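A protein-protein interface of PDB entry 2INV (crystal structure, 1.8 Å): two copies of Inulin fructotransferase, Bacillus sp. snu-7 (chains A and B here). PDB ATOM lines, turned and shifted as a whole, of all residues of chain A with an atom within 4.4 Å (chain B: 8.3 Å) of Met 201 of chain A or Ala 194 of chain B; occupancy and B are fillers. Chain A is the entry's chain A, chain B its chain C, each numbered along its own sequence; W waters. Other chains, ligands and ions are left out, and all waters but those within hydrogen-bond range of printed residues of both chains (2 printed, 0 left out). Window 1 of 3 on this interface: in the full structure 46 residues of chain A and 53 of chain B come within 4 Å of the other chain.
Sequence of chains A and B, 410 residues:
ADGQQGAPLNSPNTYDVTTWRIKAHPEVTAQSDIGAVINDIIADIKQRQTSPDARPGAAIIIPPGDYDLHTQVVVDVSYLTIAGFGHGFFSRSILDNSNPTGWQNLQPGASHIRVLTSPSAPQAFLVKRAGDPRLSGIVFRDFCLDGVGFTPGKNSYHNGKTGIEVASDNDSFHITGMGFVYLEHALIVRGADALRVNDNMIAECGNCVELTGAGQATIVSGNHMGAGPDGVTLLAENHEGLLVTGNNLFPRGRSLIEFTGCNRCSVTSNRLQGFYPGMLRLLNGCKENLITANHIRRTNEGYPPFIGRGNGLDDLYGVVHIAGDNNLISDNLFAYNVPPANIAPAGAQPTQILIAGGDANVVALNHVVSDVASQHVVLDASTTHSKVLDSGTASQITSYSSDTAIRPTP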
ATOM      1  N   HIS A  87      20.030  19.097  -4.159  1.00  0.00           N
ATOM      2  CA  HIS A  87      19.570  17.716  -3.990  1.00  0.00           C
ATOM      3  C   HIS A  87      19.299  17.067  -5.347  1.00  0.00           C
ATOM      4  O   HIS A  87      19.261  15.846  -5.471  1.00  0.00           O
ATOM      5  CB  HIS A  87      18.291  17.688  -3.145  1.00  0.00           C
ATOM      6  CG  HIS A  87      17.130  18.385  -3.780  1.00  0.00           C
ATOM      7  ND1 HIS A  87      17.112  19.743  -4.022  1.00  0.00           N
ATOM      8  CD2 HIS A  87      15.943  17.910  -4.226  1.00  0.00           C
ATOM      9  CE1 HIS A  87      15.964  20.073  -4.587  1.00  0.00           C
ATOM     10  NE2 HIS A  87      15.238  18.980  -4.722  1.00  0.00           N
ATOM     11  N   PHE A  89      16.853  16.154  -7.229  1.00  0.00           N
ATOM     12  CA  PHE A  89      16.017  14.984  -7.456  1.00  0.00           C
ATOM     13  C   PHE A  89      15.357  15.014  -8.829  1.00  0.00           C
ATOM     14  O   PHE A  89      15.074  16.077  -9.399  1.00  0.00           O
ATOM     15  CB  PHE A  89      14.940  14.820  -6.381  1.00  0.00           C
ATOM     16  CG  PHE A  89      14.072  13.608  -6.592  1.00  0.00           C
ATOM     17  CD1 PHE A  89      12.929  13.684  -7.377  1.00  0.00           C
ATOM     18  CD2 PHE A  89      14.435  12.374  -6.055  1.00  0.00           C
ATOM     19  CE1 PHE A  89      12.159  12.556  -7.633  1.00  0.00           C
ATOM     20  CE2 PHE A  89      13.671  11.231  -6.305  1.00  0.00           C
ATOM     21  CZ  PHE A  89      12.530  11.327  -7.097  1.00  0.00           C
ATOM     22  N   MET A 178      19.664  16.771   1.374  1.00  0.00           N
ATOM     23  CA  MET A 178      20.077  15.763   0.404  1.00  0.00           C
ATOM     24  C   MET A 178      19.032  15.274  -0.585  1.00  0.00           C
ATOM     25  O   MET A 178      17.826  15.537  -0.450  1.00  0.00           O
ATOM     26  CB  MET A 178      20.660  14.552   1.128  1.00  0.00           C
ATOM     27  CG  MET A 178      21.787  14.888   2.105  1.00  0.00           C
ATOM     28  SD  MET A 178      23.538  14.749   1.327  1.00  0.00           S
ATOM     29  CE  MET A 178      23.284  13.076   0.394  1.00  0.00           C
ATOM     30  N   GLY A 179      19.530  14.557  -1.588  1.00  0.00           N
ATOM     31  CA  GLY A 179      18.686  13.991  -2.618  1.00  0.00           C
ATOM     32  C   GLY A 179      19.150  12.566  -2.830  1.00  0.00           C
ATOM     33  O   GLY A 179      20.295  12.331  -3.228  1.00  0.00           O
ATOM     34  N   PHE A 180      18.279  11.611  -2.526  1.00  0.00           N
ATOM     35  CA  PHE A 180      18.597  10.197  -2.691  1.00  0.00           C
ATOM     36  C   PHE A 180      17.616   9.658  -3.713  1.00  0.00           C
ATOM     37  O   PHE A 180      16.407   9.861  -3.578  1.00  0.00           O
ATOM     38  CB  PHE A 180      18.396   9.435  -1.380  1.00  0.00           C
ATOM     39  CG  PHE A 180      19.354   9.818  -0.290  1.00  0.00           C
ATOM     40  CD1 PHE A 180      20.562   9.137  -0.121  1.00  0.00           C
ATOM     41  CD2 PHE A 180      19.023  10.823   0.606  1.00  0.00           C
ATOM     42  CE1 PHE A 180      21.413   9.450   0.928  1.00  0.00           C
ATOM     43  CE2 PHE A 180      19.872  11.142   1.660  1.00  0.00           C
ATOM     44  CZ  PHE A 180      21.065  10.456   1.826  1.00  0.00           C
ATOM     45  N   ASN A 200      15.279  16.616   3.807  1.00  0.00           N
ATOM     46  CA  ASN A 200      15.812  15.796   2.716  1.00  0.00           C
ATOM     47  C   ASN A 200      14.734  15.239   1.799  1.00  0.00           C
ATOM     48  O   ASN A 200      13.556  15.200   2.158  1.00  0.00           O
ATOM     49  CB  ASN A 200      16.637  14.608   3.246  1.00  0.00           C
ATOM     50  CG  ASN A 200      17.682  15.015   4.251  1.00  0.00           C
ATOM     51  OD1 ASN A 200      18.843  15.443   3.762  1.00  0.00           O
ATOM     52  ND2 ASN A 200      17.454  14.939   5.461  1.00  0.00           N
ATOM     53  N   MET A 201      15.171  14.796   0.621  1.00  0.00           N
ATOM     54  CA  MET A 201      14.299  14.186  -0.377  1.00  0.00           C
ATOM     55  C   MET A 201      14.843  12.796  -0.664  1.00  0.00           C
ATOM     56  O   MET A 201      15.829  12.643  -1.395  1.00  0.00           O
ATOM     57  CB  MET A 201      14.288  15.019  -1.655  1.00  0.00           C
ATOM     58  CG  MET A 201      13.600  14.360  -2.844  1.00  0.00           C
ATOM     59  SD  MET A 201      11.768  13.921  -2.520  1.00  0.00           S
ATOM     60  CE  MET A 201      10.999  15.662  -2.788  1.00  0.00           C
ATOM     61  N   ILE A 202      14.199  11.799  -0.063  1.00  0.00           N
ATOM     62  CA  ILE A 202      14.608  10.409  -0.198  1.00  0.00           C
ATOM     63  C   ILE A 202      13.466   9.630  -0.835  1.00  0.00           C
ATOM     64  O   ILE A 202      12.534   9.208  -0.137  1.00  0.00           O
ATOM     65  CB  ILE A 202      14.873   9.804   1.182  1.00  0.00           C
ATOM     66  CG1 ILE A 202      15.580  10.836   2.059  1.00  0.00           C
ATOM     67  CG2 ILE A 202      15.701   8.539   1.052  1.00  0.00           C
ATOM     68  CD1 ILE A 202      15.729  10.429   3.493  1.00  0.00           C
ATOM     69  N   ALA A 203      13.521   9.417  -2.143  1.00  0.00           N
ATOM     70  CA  ALA A 203      12.437   8.691  -2.780  1.00  0.00           C
ATOM     71  C   ALA A 203      12.857   7.815  -3.938  1.00  0.00           C
ATOM     72  O   ALA A 203      13.939   7.990  -4.522  1.00  0.00           O
ATOM     73  CB  ALA A 203      11.366   9.660  -3.229  1.00  0.00           C
ATOM     74  N   HIS A 224      10.894  14.376   2.928  1.00  0.00           N
ATOM     75  CA  HIS A 224       9.992  13.870   1.882  1.00  0.00           C
ATOM     76  C   HIS A 224      10.431  12.422   1.611  1.00  0.00           C
ATOM     77  O   HIS A 224      11.533  12.218   1.103  1.00  0.00           O
ATOM     78  CB  HIS A 224      10.197  14.649   0.575  1.00  0.00           C
ATOM     79  CG  HIS A 224       9.360  15.888   0.430  1.00  0.00           C
ATOM     80  ND1 HIS A 224       7.987  15.855   0.306  1.00  0.00           N
ATOM     81  CD2 HIS A 224       9.711  17.192   0.294  1.00  0.00           C
ATOM     82  CE1 HIS A 224       7.530  17.079   0.097  1.00  0.00           C
ATOM     83  NE2 HIS A 224       8.556  17.908   0.084  1.00  0.00           N
ATOM     84  N   ARG B 134       9.226  17.556 -16.525  1.00  0.00           N
ATOM     85  CA  ARG B 134       8.794  18.722 -15.798  1.00  0.00           C
ATOM     86  C   ARG B 134      10.070  19.164 -15.154  1.00  0.00           C
ATOM     87  O   ARG B 134      10.960  18.351 -14.888  1.00  0.00           O
ATOM     88  CB  ARG B 134       7.830  18.404 -14.678  1.00  0.00           C
ATOM     89  CG  ARG B 134       6.531  17.774 -15.068  1.00  0.00           C
ATOM     90  CD  ARG B 134       5.829  17.412 -13.772  1.00  0.00           C
ATOM     91  NE  ARG B 134       6.406  16.214 -13.172  1.00  0.00           N
ATOM     92  CZ  ARG B 134       6.121  15.775 -11.956  1.00  0.00           C
ATOM     93  NH1 ARG B 134       5.268  16.436 -11.197  1.00  0.00           N
ATOM     94  NH2 ARG B 134       6.674  14.664 -11.511  1.00  0.00           N
ATOM     95  N   GLY B 137      14.089  19.782  -9.173  1.00  0.00           N
ATOM     96  CA  GLY B 137      15.217  20.148  -8.341  1.00  0.00           C
ATOM     97  C   GLY B 137      15.670  21.593  -8.273  1.00  0.00           C
ATOM     98  O   GLY B 137      16.769  21.861  -7.793  1.00  0.00           O
ATOM     99  N   ASN B 170       6.096  21.468 -11.631  1.00  0.00           N
ATOM    100  CA  ASN B 170       7.440  21.280 -11.122  1.00  0.00           C
ATOM    101  C   ASN B 170       7.552  20.103 -10.169  1.00  0.00           C
ATOM    102  O   ASN B 170       6.570  19.691  -9.546  1.00  0.00           O
ATOM    103  CB  ASN B 170       7.836  22.541 -10.374  1.00  0.00           C
ATOM    104  CG  ASN B 170       6.741  23.002  -9.414  1.00  0.00           C
ATOM    105  OD1 ASN B 170       6.798  22.736  -8.216  1.00  0.00           O
ATOM    106  ND2 ASN B 170       5.721  23.668  -9.948  1.00  0.00           N
ATOM    107  N   ASP B 171       8.747  19.538 -10.069  1.00  0.00           N
ATOM    108  CA  ASP B 171       8.950  18.444  -9.141  1.00  0.00           C
ATOM    109  C   ASP B 171      10.171  18.651  -8.269  1.00  0.00           C
ATOM    110  O   ASP B 171      11.253  19.006  -8.736  1.00  0.00           O
ATOM    111  CB  ASP B 171       9.083  17.112  -9.859  1.00  0.00           C
ATOM    112  CG  ASP B 171       9.084  15.948  -8.888  1.00  0.00           C
ATOM    113  OD1 ASP B 171       8.341  16.017  -7.878  1.00  0.00           O
ATOM    114  OD2 ASP B 171       9.835  14.971  -9.113  1.00  0.00           O
ATOM    115  N   SER B 172       9.950  18.441  -6.980  1.00  0.00           N
ATOM    116  CA  SER B 172      10.970  18.549  -5.957  1.00  0.00           C
ATOM    117  C   SER B 172      11.641  19.916  -5.850  1.00  0.00           C
ATOM    118  O   SER B 172      12.860  19.997  -5.696  1.00  0.00           O
ATOM    119  CB  SER B 172      12.033  17.479  -6.183  1.00  0.00           C
ATOM    120  OG  SER B 172      12.733  17.219  -4.980  1.00  0.00           O
ATOM    121  N   PHE B 173      10.865  20.993  -5.914  1.00  0.00           N
ATOM    122  CA  PHE B 173      11.462  22.315  -5.787  1.00  0.00           C
ATOM    123  C   PHE B 173      11.742  22.565  -4.315  1.00  0.00           C
ATOM    124  O   PHE B 173      11.093  21.971  -3.449  1.00  0.00           O
ATOM    125  CB  PHE B 173      10.532  23.386  -6.359  1.00  0.00           C
ATOM    126  CG  PHE B 173      10.718  23.616  -7.841  1.00  0.00           C
ATOM    127  CD1 PHE B 173      11.080  22.569  -8.680  1.00  0.00           C
ATOM    128  CD2 PHE B 173      10.504  24.868  -8.398  1.00  0.00           C
ATOM    129  CE1 PHE B 173      11.224  22.760 -10.045  1.00  0.00           C
ATOM    130  CE2 PHE B 173      10.644  25.073  -9.766  1.00  0.00           C
ATOM    131  CZ  PHE B 173      11.003  24.023 -10.595  1.00  0.00           C
ATOM    132  N   HIS B 174      12.720  23.424  -4.041  1.00  0.00           N
ATOM    133  CA  HIS B 174      13.109  23.753  -2.678  1.00  0.00           C
ATOM    134  C   HIS B 174      13.297  25.259  -2.550  1.00  0.00           C
ATOM    135  O   HIS B 174      14.099  25.859  -3.262  1.00  0.00           O
ATOM    136  CB  HIS B 174      14.407  23.013  -2.336  1.00  0.00           C
ATOM    137  CG  HIS B 174      14.718  22.958  -0.875  1.00  0.00           C
ATOM    138  ND1 HIS B 174      13.890  23.494   0.088  1.00  0.00           N
ATOM    139  CD2 HIS B 174      15.742  22.373  -0.206  1.00  0.00           C
ATOM    140  CE1 HIS B 174      14.389  23.244   1.285  1.00  0.00           C
ATOM    141  NE2 HIS B 174      15.511  22.566   1.134  1.00  0.00           N
ATOM    142  N   ILE B 175      12.550  25.859  -1.631  1.00  0.00           N
ATOM    143  CA  ILE B 175      12.604  27.298  -1.381  1.00  0.00           C
ATOM    144  C   ILE B 175      12.928  27.515   0.093  1.00  0.00           C
ATOM    145  O   ILE B 175      12.041  27.422   0.933  1.00  0.00           O
ATOM    146  CB  ILE B 175      11.235  27.963  -1.650  1.00  0.00           C
ATOM    147  CG1 ILE B 175      10.755  27.653  -3.070  1.00  0.00           C
ATOM    148  CG2 ILE B 175      11.336  29.469  -1.422  1.00  0.00           C
ATOM    149  CD1 ILE B 175      11.592  28.293  -4.176  1.00  0.00           C
ATOM    150  N   GLY B 191       1.015  23.926  -9.768  1.00  0.00           N
ATOM    151  CA  GLY B 191       1.333  22.530 -10.036  1.00  0.00           C
ATOM    152  C   GLY B 191       2.566  22.023  -9.317  1.00  0.00           C
ATOM    153  O   GLY B 191       3.427  21.374  -9.907  1.00  0.00           O
ATOM    154  N   ALA B 192       2.644  22.328  -8.027  1.00  0.00           N
ATOM    155  CA  ALA B 192       3.769  21.913  -7.198  1.00  0.00           C
ATOM    156  C   ALA B 192       3.601  20.461  -6.782  1.00  0.00           C
ATOM    157  O   ALA B 192       2.496  20.012  -6.452  1.00  0.00           O
ATOM    158  CB  ALA B 192       3.876  22.801  -5.975  1.00  0.00           C
ATOM    159  N   ASP B 193       4.714  19.736  -6.801  1.00  0.00           N
ATOM    160  CA  ASP B 193       4.735  18.318  -6.463  1.00  0.00           C
ATOM    161  C   ASP B 193       6.014  18.079  -5.642  1.00  0.00           C
ATOM    162  O   ASP B 193       7.124  18.303  -6.135  1.00  0.00           O
ATOM    163  CB  ASP B 193       4.789  17.511  -7.752  1.00  0.00           C
ATOM    164  CG  ASP B 193       4.783  16.021  -7.515  1.00  0.00           C
ATOM    165  OD1 ASP B 193       4.544  15.580  -6.368  1.00  0.00           O
ATOM    166  OD2 ASP B 193       5.070  15.267  -8.472  1.00  0.00           O
ATOM    167  N   ALA B 194       5.855  17.648  -4.391  1.00  0.00           N
ATOM    168  CA  ALA B 194       6.981  17.395  -3.486  1.00  0.00           C
ATOM    169  C   ALA B 194       7.778  18.674  -3.279  1.00  0.00           C
ATOM    170  O   ALA B 194       9.006  18.648  -3.148  1.00  0.00           O
ATOM    171  CB  ALA B 194       7.878  16.304  -4.047  1.00  0.00           C
ATOM    172  N   LEU B 195       7.061  19.794  -3.265  1.00  0.00           N
ATOM    173  CA  LEU B 195       7.671  21.098  -3.074  1.00  0.00           C
ATOM    174  C   LEU B 195       7.973  21.343  -1.618  1.00  0.00           C
ATOM    175  O   LEU B 195       7.279  20.857  -0.727  1.00  0.00           O
ATOM    176  CB  LEU B 195       6.745  22.215  -3.560  1.00  0.00           C
ATOM    177  CG  LEU B 195       7.109  23.614  -3.039  1.00  0.00           C
ATOM    178  CD1 LEU B 195       8.344  24.127  -3.757  1.00  0.00           C
ATOM    179  CD2 LEU B 195       5.945  24.558  -3.247  1.00  0.00           C
ATOM    180  N   ARG B 196       9.024  22.108  -1.384  1.00  0.00           N
ATOM    181  CA  ARG B 196       9.368  22.442  -0.035  1.00  0.00           C
ATOM    182  C   ARG B 196       9.616  23.916   0.104  1.00  0.00           C
ATOM    183  O   ARG B 196      10.451  24.501  -0.596  1.00  0.00           O
ATOM    184  CB  ARG B 196      10.580  21.668   0.428  1.00  0.00           C
ATOM    185  CG  ARG B 196      10.200  20.525   1.321  1.00  0.00           C
ATOM    186  CD  ARG B 196      11.436  19.804   1.698  1.00  0.00           C
ATOM    187  NE  ARG B 196      12.076  19.280   0.503  1.00  0.00           N
ATOM    188  CZ  ARG B 196      13.384  19.088   0.397  1.00  0.00           C
ATOM    189  NH1 ARG B 196      14.193  19.383   1.416  1.00  0.00           N
ATOM    190  NH2 ARG B 196      13.890  18.590  -0.721  1.00  0.00           N
ATOM    191  N   VAL B 197       8.856  24.496   1.017  1.00  0.00           N
ATOM    192  CA  VAL B 197       8.915  25.897   1.341  1.00  0.00           C
ATOM    193  C   VAL B 197       9.103  25.868   2.850  1.00  0.00           C
ATOM    194  O   VAL B 197       8.155  25.644   3.596  1.00  0.00           O
ATOM    195  CB  VAL B 197       7.587  26.564   0.945  1.00  0.00           C
ATOM    196  CG1 VAL B 197       7.568  28.011   1.367  1.00  0.00           C
ATOM    197  CG2 VAL B 197       7.378  26.449  -0.561  1.00  0.00           C
ATOM    198  N   GLY B 215      -1.795  20.419  -6.565  1.00  0.00           N
ATOM    199  CA  GLY B 215      -0.555  19.980  -5.959  1.00  0.00           C
ATOM    200  C   GLY B 215      -0.609  18.660  -5.224  1.00  0.00           C
ATOM    201  O   GLY B 215      -1.678  18.114  -4.952  1.00  0.00           O
ATOM    202  N   GLN B 216       0.576  18.146  -4.919  1.00  0.00           N
ATOM    203  CA  GLN B 216       0.720  16.891  -4.198  1.00  0.00           C
ATOM    204  C   GLN B 216       1.944  16.894  -3.288  1.00  0.00           C
ATOM    205  O   GLN B 216       2.956  17.529  -3.589  1.00  0.00           O
ATOM    206  CB  GLN B 216       0.831  15.706  -5.165  1.00  0.00           C
ATOM    207  CG  GLN B 216      -0.271  14.682  -5.056  1.00  0.00           C
ATOM    208  CD  GLN B 216      -1.116  14.623  -6.306  1.00  0.00           C
ATOM    209  OE1 GLN B 216      -0.648  14.212  -7.375  1.00  0.00           O
ATOM    210  NE2 GLN B 216      -2.369  15.051  -6.188  1.00  0.00           N
ATOM    211  N   ALA B 217       1.826  16.158  -2.183  1.00  0.00           N
ATOM    212  CA  ALA B 217       2.874  16.003  -1.175  1.00  0.00           C
ATOM    213  C   ALA B 217       3.818  17.189  -1.062  1.00  0.00           C
ATOM    214  O   ALA B 217       5.022  17.073  -1.288  1.00  0.00           O
ATOM    215  CB  ALA B 217       3.662  14.741  -1.443  1.00  0.00           C
ATOM    216  N   THR B 218       3.262  18.324  -0.670  1.00  0.00           N
ATOM    217  CA  THR B 218       4.027  19.541  -0.502  1.00  0.00           C
ATOM    218  C   THR B 218       4.160  19.821   0.989  1.00  0.00           C
ATOM    219  O   THR B 218       3.298  19.447   1.776  1.00  0.00           O
ATOM    220  CB  THR B 218       3.319  20.719  -1.209  1.00  0.00           C
ATOM    221  OG1 THR B 218       3.284  20.464  -2.621  1.00  0.00           O
ATOM    222  CG2 THR B 218       4.040  22.020  -0.937  1.00  0.00           C
ATOM    223  N   ILE B 219       5.253  20.468   1.372  1.00  0.00           N
ATOM    224  CA  ILE B 219       5.493  20.810   2.764  1.00  0.00           C
ATOM    225  C   ILE B 219       5.799  22.288   2.912  1.00  0.00           C
ATOM    226  O   ILE B 219       6.682  22.815   2.236  1.00  0.00           O
ATOM    227  CB  ILE B 219       6.686  20.025   3.359  1.00  0.00           C
ATOM    228  CG1 ILE B 219       6.393  18.520   3.367  1.00  0.00           C
ATOM    229  CG2 ILE B 219       6.960  20.520   4.771  1.00  0.00           C
ATOM    230  CD1 ILE B 219       7.558  17.685   3.826  1.00  0.00           C
ATOM    231  N   HIS B 239      -4.936  20.979  -3.602  1.00  0.00           N
ATOM    232  CA  HIS B 239      -3.756  20.276  -3.130  1.00  0.00           C
ATOM    233  C   HIS B 239      -4.180  19.039  -2.378  1.00  0.00           C
ATOM    234  O   HIS B 239      -5.252  18.990  -1.771  1.00  0.00           O
ATOM    235  CB  HIS B 239      -2.914  21.156  -2.208  1.00  0.00           C
ATOM    236  CG  HIS B 239      -1.758  21.811  -2.893  1.00  0.00           C
ATOM    237  ND1 HIS B 239      -0.446  21.504  -2.606  1.00  0.00           N
ATOM    238  CD2 HIS B 239      -1.717  22.768  -3.853  1.00  0.00           C
ATOM    239  CE1 HIS B 239       0.352  22.242  -3.354  1.00  0.00           C
ATOM    240  NE2 HIS B 239      -0.394  23.017  -4.120  1.00  0.00           N
ATOM    241  N   GLU B 240      -3.305  18.050  -2.411  1.00  0.00           N
ATOM    242  CA  GLU B 240      -3.535  16.787  -1.759  1.00  0.00           C
ATOM    243  C   GLU B 240      -2.226  16.464  -1.063  1.00  0.00           C
ATOM    244  O   GLU B 240      -1.158  16.615  -1.650  1.00  0.00           O
ATOM    245  CB  GLU B 240      -3.863  15.751  -2.821  1.00  0.00           C
ATOM    246  CG  GLU B 240      -3.731  14.302  -2.394  1.00  0.00           C
ATOM    247  CD  GLU B 240      -5.055  13.688  -2.002  1.00  0.00           C
ATOM    248  OE1 GLU B 240      -6.109  14.242  -2.377  1.00  0.00           O
ATOM    249  OE2 GLU B 240      -5.040  12.625  -1.347  1.00  0.00           O
ATOM    250  N   GLY B 241      -2.305  16.055   0.200  1.00  0.00           N
ATOM    251  CA  GLY B 241      -1.103  15.729   0.951  1.00  0.00           C
ATOM    252  C   GLY B 241      -0.289  16.926   1.418  1.00  0.00           C
ATOM    253  O   GLY B 241       0.893  16.781   1.732  1.00  0.00           O
HETATM  254  O   HOH W   1      16.676  18.219  -0.150  1.00  0.00           O
HETATM  255  O   HOH W   2      19.003  20.591  -6.991  1.00  0.00           O
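Of the 10 printed residues of chain A, 5 touch a printed residue of chain B. Hydrophobic or aromatic side chains of chain A within 4 Å of the printed part of chain B: His 87, Phe 89, Met 201 and His 224. Among the printed residues, 14 pairs touch across the chains. Among the printed residues, no Asp or Glu carboxylate lies within 4 Å of a Lys or Arg side-chain nitrogen of the other chain.
A ring nitrogen (NE2) of His 87 of chain A lies within hydrogen-bond range of the backbone carbonyl oxygen of Ser 172 of chain B. NE2 of His 224 of chain A sits at hydrogen-bond distance from O of Ala 194 of chain B. A ring nitrogen (NE2) of His 224 of chain A sits at hydrogen-bond distance from the backbone carbonyl oxygen (O) of Leu 195 of chain B, at 3.3 Å.
The backbone NH of Met 178 of chain A sits at hydrogen-bond distance from the side-chain amide oxygen of Asn 200 of chain A. The backbone carbonyl oxygen of Asp 193 of chain B lies within hydrogen-bond range of the backbone NH of Ser 172 of chain B, at 3.0 Å. N of Arg 196 of chain B is in hydrogen-bond range of O of Phe 173 of chain B, 2.9 Å away. O of Gln 216 of chain B sits at hydrogen-bond distance from N of Ala 194 of chain B. The backbone NH (N) of Ala 194 of chain B sits close to the backbone carbonyl oxygen (O) of Ala 217 of chain B (3.3 Å). The backbone carbonyl oxygen (O) of Leu 195 of chain B sits at hydrogen-bond distance from the backbone NH (N) of Ile 219 of chain B, at 2.9 Å.
No position is printed for both chains.
Of chain B, only Ser 172, Ala 194 and Arg 196 come within 4 Å of Met 201 of chain A. Of chain A, only Met 201 and His 224 come within 4 Å of Ala 194 of chain B. Of the printed residues of chain B, Phe 89 of chain A touches Gly 137 (3.8 Å), Asp 171 (3.7 Å) and Ser 172 (3.5 Å). Of the printed residues of chain B, Asn 200 of chain A touches Arg 196. The nearest printed residue of chain B that does not touch Met 201 of chain A is Leu 195 of chain B (5.7 Å). The nearest printed residue of chain A that does not touch Ala 194 of chain B is His 87 of chain A (6.4 Å). The nearest printed residue of chain B that does not touch His 87 of chain A is His 174 of chain B (4.02 Å).
Among the printed residues, pairs that only touch across the chains: His 224 of chain A with Ala 217 of chain B, His 224 of chain A with Arg 196 of chain B, Met 201 of chain A with Ser 172 of chain B, Met 201 of chain A with Ala 194 of chain B, Phe 89 of chain A with Ser 172 of chain B, Phe 89 of chain A with Asp 171 of chain B, Met 201 of chain A with Arg 196 of chain B, His 224 of chain A with Ile 219 of chain B, His 87 of chain A with Gly 137 of chain B, Asn 200 of chain A with Arg 196 of chain B and Phe 89 of chain A with Gly 137 of chain B.
Water W2 lies within hydrogen-bond range of O of Gly 137 of chain B (2.7 Å) and N of His 87 of chain A (3.4 Å). Water W1 bridges NH2 of Arg 196 of chain B and O of Met 178 of chain A.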
